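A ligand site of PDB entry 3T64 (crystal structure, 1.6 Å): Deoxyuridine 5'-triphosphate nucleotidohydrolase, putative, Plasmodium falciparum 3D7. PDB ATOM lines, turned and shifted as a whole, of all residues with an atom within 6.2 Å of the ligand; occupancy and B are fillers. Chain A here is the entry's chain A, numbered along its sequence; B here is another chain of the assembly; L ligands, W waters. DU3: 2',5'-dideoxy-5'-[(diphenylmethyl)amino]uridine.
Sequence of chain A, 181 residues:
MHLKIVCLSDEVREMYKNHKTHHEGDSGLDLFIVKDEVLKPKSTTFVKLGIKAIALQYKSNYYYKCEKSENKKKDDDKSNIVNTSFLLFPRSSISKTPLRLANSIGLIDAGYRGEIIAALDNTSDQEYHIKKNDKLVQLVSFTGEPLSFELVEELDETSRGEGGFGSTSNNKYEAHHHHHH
N of Ile 117 is in hydrogen-bond range of O2 of the ligand (3.0 Å). The backbone carbonyl oxygen (O) of Ile 117 is in hydrogen-bond range of a nitrogen (N3) of the ligand, at 2.8 Å. ND2 of Asn 103 sits at hydrogen-bond distance from O4 of the ligand, at 3.0 Å. The side-chain hydroxyl of Tyr 112 sits at hydrogen-bond distance from an oxygen (O4') of the ligand, 3.5 Å away.
O of Gly 106 lies within hydrogen-bond range of N of Leu 88. O of Ser 92 of chain B is in hydrogen-bond range of OG of Ser 95 of chain B (2.8 Å). The backbone carbonyl oxygen (O) of Glu 115 sits at hydrogen-bond distance from the side-chain hydroxyl (OH) of Tyr 112 (2.6 Å).
Merely in contact with the ligand: Lys 96 of chain B, Gly 106, Ser 92 of chain B, Ile 108, Leu 88, Phe 46, Ser 95 of chain B, Ala 119, Ile 116, Leu 107 and Glu 115. Hydrophobic or aromatic side chains within 4 Å of the ligand: Phe 46, Leu 88, Ile 108, Tyr 112, Ile 117 and Ala 119. The nearest printed residue that does not touch the ligand is Ser 93 of chain B (4.8 Å).
Water W4 lies within hydrogen-bond range of OD1 of Asn 103 (2.8 Å), O4 of the ligand (2.8 Å) and N of Ala 119 (2.9 Å). Water W2 bridges the side-chain carboxylate of Asp 109 (2.6 Å) and an oxygen (O3') of the ligand (3.4 Å). Water W1 lies within hydrogen-bond range of the backbone NH of Leu 107 and the side-chain amide nitrogen of Asn 103.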
ATOM      1  N   PHE A  46      -1.390  13.538   7.890  1.00  0.00           N
ATOM      2  CA  PHE A  46      -0.248  12.944   7.178  1.00  0.00           C
ATOM      3  C   PHE A  46       0.194  13.935   6.108  1.00  0.00           C
ATOM      4  O   PHE A  46      -0.381  14.000   5.001  1.00  0.00           O
ATOM      5  CB  PHE A  46      -0.620  11.560   6.651  1.00  0.00           C
ATOM      6  CG  PHE A  46      -0.949  10.598   7.755  1.00  0.00           C
ATOM      7  CD1 PHE A  46      -2.236  10.547   8.302  1.00  0.00           C
ATOM      8  CD2 PHE A  46       0.037   9.800   8.303  1.00  0.00           C
ATOM      9  CE1 PHE A  46      -2.517   9.669   9.364  1.00  0.00           C
ATOM     10  CE2 PHE A  46      -0.237   8.929   9.342  1.00  0.00           C
ATOM     11  CZ  PHE A  46      -1.517   8.867   9.892  1.00  0.00           C
ATOM     12  N   LEU A  88      13.691  10.055  10.192  1.00  0.00           N
ATOM     13  CA  LEU A  88      13.021  11.330  10.121  1.00  0.00           C
ATOM     14  C   LEU A  88      12.810  11.842  11.566  1.00  0.00           C
ATOM     15  O   LEU A  88      12.055  11.263  12.320  1.00  0.00           O
ATOM     16  CB  LEU A  88      11.692  11.154   9.391  1.00  0.00           C
ATOM     17  CG  LEU A  88      10.841  12.439   9.235  1.00  0.00           C
ATOM     18  CD1 LEU A  88      11.453  13.466   8.293  1.00  0.00           C
ATOM     19  CD2 LEU A  88       9.410  12.117   8.754  1.00  0.00           C
ATOM     20  N   LEU A 101       5.448  14.843  16.397  1.00  0.00           N
ATOM     21  CA  LEU A 101       5.530  13.734  15.437  1.00  0.00           C
ATOM     22  C   LEU A 101       4.901  12.472  16.035  1.00  0.00           C
ATOM     23  O   LEU A 101       5.363  11.958  17.058  1.00  0.00           O
ATOM     24  CB  LEU A 101       7.000  13.457  15.030  1.00  0.00           C
ATOM     25  CG  LEU A 101       7.150  12.784  13.658  1.00  0.00           C
ATOM     26  CD1 LEU A 101       6.754  13.699  12.525  1.00  0.00           C
ATOM     27  CD2 LEU A 101       8.618  12.415  13.564  1.00  0.00           C
ATOM     28  N   ASN A 103       4.665   9.276  15.298  1.00  0.00           N
ATOM     29  CA  ASN A 103       5.452   8.054  15.452  1.00  0.00           C
ATOM     30  C   ASN A 103       6.828   8.256  16.110  1.00  0.00           C
ATOM     31  O   ASN A 103       7.690   7.369  16.057  1.00  0.00           O
ATOM     32  CB  ASN A 103       5.562   7.327  14.098  1.00  0.00           C
ATOM     33  CG  ASN A 103       6.096   8.212  13.000  1.00  0.00           C
ATOM     34  OD1 ASN A 103       5.841   9.424  12.962  1.00  0.00           O
ATOM     35  ND2 ASN A 103       6.832   7.606  12.060  1.00  0.00           N
ATOM     36  N   ILE A 105       9.887   9.091  15.958  1.00  0.00           N
ATOM     37  CA  ILE A 105      10.986   9.222  14.980  1.00  0.00           C
ATOM     38  C   ILE A 105      10.611   8.285  13.837  1.00  0.00           C
ATOM     39  O   ILE A 105      10.248   7.128  14.077  1.00  0.00           O
ATOM     40  CB  ILE A 105      12.360   8.775  15.576  1.00  0.00           C
ATOM     41  CG1 ILE A 105      12.752   9.562  16.845  1.00  0.00           C
ATOM     42  CG2 ILE A 105      13.466   8.832  14.469  1.00  0.00           C
ATOM     43  CD1 ILE A 105      13.084  11.050  16.612  1.00  0.00           C
ATOM     44  N   GLY A 106      10.686   8.769  12.606  1.00  0.00           N
ATOM     45  CA  GLY A 106      10.268   7.960  11.433  1.00  0.00           C
ATOM     46  C   GLY A 106      11.445   7.136  10.980  1.00  0.00           C
ATOM     47  O   GLY A 106      12.581   7.618  10.938  1.00  0.00           O
ATOM     48  N   LEU A 107      11.167   5.880  10.648  1.00  0.00           N
ATOM     49  CA  LEU A 107      12.192   4.966  10.170  1.00  0.00           C
ATOM     50  C   LEU A 107      11.875   4.713   8.701  1.00  0.00           C
ATOM     51  O   LEU A 107      10.837   4.127   8.366  1.00  0.00           O
ATOM     52  CB  LEU A 107      12.182   3.672  10.978  1.00  0.00           C
ATOM     53  CG  LEU A 107      13.444   2.790  10.923  1.00  0.00           C
ATOM     54  CD1 LEU A 107      13.238   1.533  11.744  1.00  0.00           C
ATOM     55  CD2 LEU A 107      13.821   2.408   9.495  1.00  0.00           C
ATOM     56  N   ILE A 108      12.765   5.171   7.825  1.00  0.00           N
ATOM     57  CA  ILE A 108      12.560   5.026   6.379  1.00  0.00           C
ATOM     58  C   ILE A 108      13.433   3.864   5.952  1.00  0.00           C
ATOM     59  O   ILE A 108      14.637   3.997   5.973  1.00  0.00           O
ATOM     60  CB  ILE A 108      12.993   6.311   5.591  1.00  0.00           C
ATOM     61  CG1 ILE A 108      12.408   7.594   6.222  1.00  0.00           C
ATOM     62  CG2 ILE A 108      12.592   6.188   4.102  1.00  0.00           C
ATOM     63  CD1 ILE A 108      10.921   7.664   6.172  1.00  0.00           C
ATOM     64  N   ASP A 109      12.848   2.729   5.592  1.00  0.00           N
ATOM     65  CA  ASP A 109      13.675   1.573   5.227  1.00  0.00           C
ATOM     66  C   ASP A 109      14.347   1.799   3.872  1.00  0.00           C
ATOM     67  O   ASP A 109      13.833   2.554   3.032  1.00  0.00           O
ATOM     68  CB  ASP A 109      12.848   0.282   5.231  1.00  0.00           C
ATOM     69  CG  ASP A 109      12.319  -0.071   6.609  1.00  0.00           C
ATOM     70  OD1 ASP A 109      13.082  -0.658   7.420  1.00  0.00           O
ATOM     71  OD2 ASP A 109      11.140   0.253   6.892  1.00  0.00           O
ATOM     72  N   TYR A 112      12.231   1.909   0.480  1.00  0.00           N
ATOM     73  CA  TYR A 112      11.060   2.755   0.331  1.00  0.00           C
ATOM     74  C   TYR A 112      11.279   3.752  -0.809  1.00  0.00           C
ATOM     75  O   TYR A 112      12.287   4.468  -0.832  1.00  0.00           O
ATOM     76  CB  TYR A 112      10.724   3.487   1.644  1.00  0.00           C
ATOM     77  CG  TYR A 112       9.495   4.353   1.570  1.00  0.00           C
ATOM     78  CD1 TYR A 112       8.216   3.785   1.460  1.00  0.00           C
ATOM     79  CD2 TYR A 112       9.594   5.743   1.644  1.00  0.00           C
ATOM     80  CE1 TYR A 112       7.068   4.594   1.400  1.00  0.00           C
ATOM     81  CE2 TYR A 112       8.466   6.541   1.593  1.00  0.00           C
ATOM     82  CZ  TYR A 112       7.196   5.969   1.480  1.00  0.00           C
ATOM     83  OH  TYR A 112       6.076   6.774   1.406  1.00  0.00           O
ATOM     84  N   GLY A 114       8.372   5.612  -1.782  1.00  0.00           N
ATOM     85  CA  GLY A 114       7.218   6.500  -1.756  1.00  0.00           C
ATOM     86  C   GLY A 114       7.580   7.915  -1.309  1.00  0.00           C
ATOM     87  O   GLY A 114       8.692   8.179  -0.892  1.00  0.00           O
ATOM     88  N   GLU A 115       6.605   8.816  -1.384  1.00  0.00           N
ATOM     89  CA  GLU A 115       6.778  10.182  -0.887  1.00  0.00           C
ATOM     90  C   GLU A 115       7.046  10.170   0.622  1.00  0.00           C
ATOM     91  O   GLU A 115       6.407   9.401   1.361  1.00  0.00           O
ATOM     92  CB  GLU A 115       5.527  10.999  -1.182  1.00  0.00           C
ATOM     93  CG  GLU A 115       5.654  12.483  -0.893  1.00  0.00           C
ATOM     94  CD  GLU A 115       4.496  13.263  -1.459  1.00  0.00           C
ATOM     95  OE1 GLU A 115       4.535  14.502  -1.398  1.00  0.00           O
ATOM     96  OE2 GLU A 115       3.556  12.640  -2.015  1.00  0.00           O
ATOM     97  N   ILE A 116       7.931  11.045   1.075  1.00  0.00           N
ATOM     98  CA  ILE A 116       8.204  11.150   2.505  1.00  0.00           C
ATOM     99  C   ILE A 116       7.088  11.978   3.146  1.00  0.00           C
ATOM    100  O   ILE A 116       6.709  13.042   2.664  1.00  0.00           O
ATOM    101  CB  ILE A 116       9.590  11.731   2.795  1.00  0.00           C
ATOM    102  CG1 ILE A 116      10.654  10.862   2.120  1.00  0.00           C
ATOM    103  CG2 ILE A 116       9.829  11.804   4.307  1.00  0.00           C
ATOM    104  CD1 ILE A 116      12.033  11.430   2.223  1.00  0.00           C
ATOM    105  N   ILE A 117       6.551  11.427   4.230  1.00  0.00           N
ATOM    106  CA  ILE A 117       5.391  12.002   4.912  1.00  0.00           C
ATOM    107  C   ILE A 117       5.738  12.240   6.386  1.00  0.00           C
ATOM    108  O   ILE A 117       6.426  11.425   7.029  1.00  0.00           O
ATOM    109  CB  ILE A 117       4.185  11.040   4.758  1.00  0.00           C
ATOM    110  CG1 ILE A 117       3.615  11.157   3.336  1.00  0.00           C
ATOM    111  CG2 ILE A 117       3.080  11.339   5.796  1.00  0.00           C
ATOM    112  CD1 ILE A 117       2.933   9.932   2.866  1.00  0.00           C
ATOM    113  N   ALA A 118       5.288  13.371   6.940  1.00  0.00           N
ATOM    114  CA  ALA A 118       5.371  13.621   8.391  1.00  0.00           C
ATOM    115  C   ALA A 118       3.968  13.501   8.998  1.00  0.00           C
ATOM    116  O   ALA A 118       3.074  14.230   8.586  1.00  0.00           O
ATOM    117  CB  ALA A 118       5.929  15.019   8.652  1.00  0.00           C
ATOM    118  N   ALA A 119       3.792  12.551   9.910  1.00  0.00           N
ATOM    119  CA  ALA A 119       2.510  12.385  10.608  1.00  0.00           C
ATOM    120  C   ALA A 119       2.516  13.319  11.813  1.00  0.00           C
ATOM    121  O   ALA A 119       3.218  13.065  12.793  1.00  0.00           O
ATOM    122  CB  ALA A 119       2.355  10.925  11.077  1.00  0.00           C
ATOM    123  N   SER B  92       5.361   2.992  12.250  1.00  0.00           N
ATOM    124  CA  SER B  92       4.752   4.168  11.634  1.00  0.00           C
ATOM    125  C   SER B  92       3.232   4.096  11.722  1.00  0.00           C
ATOM    126  O   SER B  92       2.567   5.096  11.877  1.00  0.00           O
ATOM    127  CB  SER B  92       5.210   4.391  10.182  1.00  0.00           C
ATOM    128  OG  SER B  92       4.703   3.356   9.341  1.00  0.00           O
ATOM    129  N   SER B  93       2.682   2.885  11.656  1.00  0.00           N
ATOM    130  CA  SER B  93       1.230   2.714  11.701  1.00  0.00           C
ATOM    131  C   SER B  93       0.605   3.027  13.055  1.00  0.00           C
ATOM    132  O   SER B  93      -0.625   3.114  13.148  1.00  0.00           O
ATOM    133  CB  SER B  93       0.846   1.284  11.277  1.00  0.00           C
ATOM    134  OG  SER B  93       1.437   0.322  12.152  1.00  0.00           O
ATOM    135  N   SER B  95       0.573   5.750  14.201  1.00  0.00           N
ATOM    136  CA  SER B  95       0.062   7.095  13.950  1.00  0.00           C
ATOM    137  C   SER B  95      -1.434   7.104  13.667  1.00  0.00           C
ATOM    138  O   SER B  95      -2.103   8.097  13.895  1.00  0.00           O
ATOM    139  CB  SER B  95       0.808   7.760  12.788  1.00  0.00           C
ATOM    140  OG  SER B  95       2.210   7.691  12.967  1.00  0.00           O
ATOM    141  N   LYS B  96      -1.938   5.981  13.145  1.00  0.00           N
ATOM    142  CA  LYS B  96      -3.366   5.840  12.785  1.00  0.00           C
ATOM    143  C   LYS B  96      -4.250   5.521  13.993  1.00  0.00           C
ATOM    144  O   LYS B  96      -5.505   5.505  13.861  1.00  0.00           O
ATOM    145  CB  LYS B  96      -3.525   4.712  11.768  1.00  0.00           C
ATOM    146  CG  LYS B  96      -2.715   4.908  10.496  1.00  0.00           C
ATOM    147  CD  LYS B  96      -2.814   3.644   9.650  1.00  0.00           C
ATOM    148  CE  LYS B  96      -2.454   3.944   8.207  1.00  0.00           C
ATOM    149  NZ  LYS B  96      -0.990   4.137   8.061  1.00  0.00           N
HETATM  150  N1  DU3 L   1       7.649   6.764   6.281  1.00  0.00           N
HETATM  151  C2  DU3 L   1       7.481   8.139   6.178  1.00  0.00           C
HETATM  152  O2  DU3 L   1       7.300   8.667   5.085  1.00  0.00           O
HETATM  153  N3  DU3 L   1       7.530   8.923   7.334  1.00  0.00           N
HETATM  154  C4  DU3 L   1       7.724   8.323   8.572  1.00  0.00           C
HETATM  155  O4  DU3 L   1       7.750   9.054   9.550  1.00  0.00           O
HETATM  156  C5  DU3 L   1       7.904   6.942   8.685  1.00  0.00           C
HETATM  157  C6  DU3 L   1       7.850   6.152   7.522  1.00  0.00           C
HETATM  158  C1' DU3 L   1       7.543   5.981   5.011  1.00  0.00           C
HETATM  159  C17 DU3 L   1       2.211   5.839   6.194  1.00  0.00           C
HETATM  160  C18 DU3 L   1       1.009   6.666   5.677  1.00  0.00           C
HETATM  161  C19 DU3 L   1      -0.179   6.641   6.401  1.00  0.00           C
HETATM  162  C2' DU3 L   1       7.972   4.536   5.176  1.00  0.00           C
HETATM  163  C20 DU3 L   1      -1.290   7.373   5.984  1.00  0.00           C
HETATM  164  C21 DU3 L   1      -1.201   8.155   4.845  1.00  0.00           C
HETATM  165  C22 DU3 L   1      -0.002   8.198   4.130  1.00  0.00           C
HETATM  166  C23 DU3 L   1       1.094   7.458   4.549  1.00  0.00           C
HETATM  167  C24 DU3 L   1       2.892   6.738   7.206  1.00  0.00           C
HETATM  168  C25 DU3 L   1       2.649   6.534   8.557  1.00  0.00           C
HETATM  169  C26 DU3 L   1       3.273   7.359   9.490  1.00  0.00           C
HETATM  170  C27 DU3 L   1       4.112   8.393   9.086  1.00  0.00           C
HETATM  171  C28 DU3 L   1       4.337   8.605   7.741  1.00  0.00           C
HETATM  172  C29 DU3 L   1       3.734   7.787   6.790  1.00  0.00           C
HETATM  173  C3' DU3 L   1       6.681   3.782   5.405  1.00  0.00           C
HETATM  174  O3' DU3 L   1       6.766   2.531   4.694  1.00  0.00           O
HETATM  175  C4' DU3 L   1       5.572   4.623   4.797  1.00  0.00           C
HETATM  176  O4' DU3 L   1       6.109   5.984   4.788  1.00  0.00           O
HETATM  177  C5' DU3 L   1       4.205   4.431   5.588  1.00  0.00           C
HETATM  178  N5' DU3 L   1       3.143   5.383   5.121  1.00  0.00           N
HETATM  179  O   HOH W   1       8.553   4.740  11.208  1.00  0.00           O
HETATM  180  O   HOH W   2      10.135   1.996   5.206  1.00  0.00           O
HETATM  181  O   HOH W   3       5.863   0.747   6.452  1.00  0.00           O
HETATM  182  O   HOH W   4       6.051  10.958  10.686  1.00  0.00           O
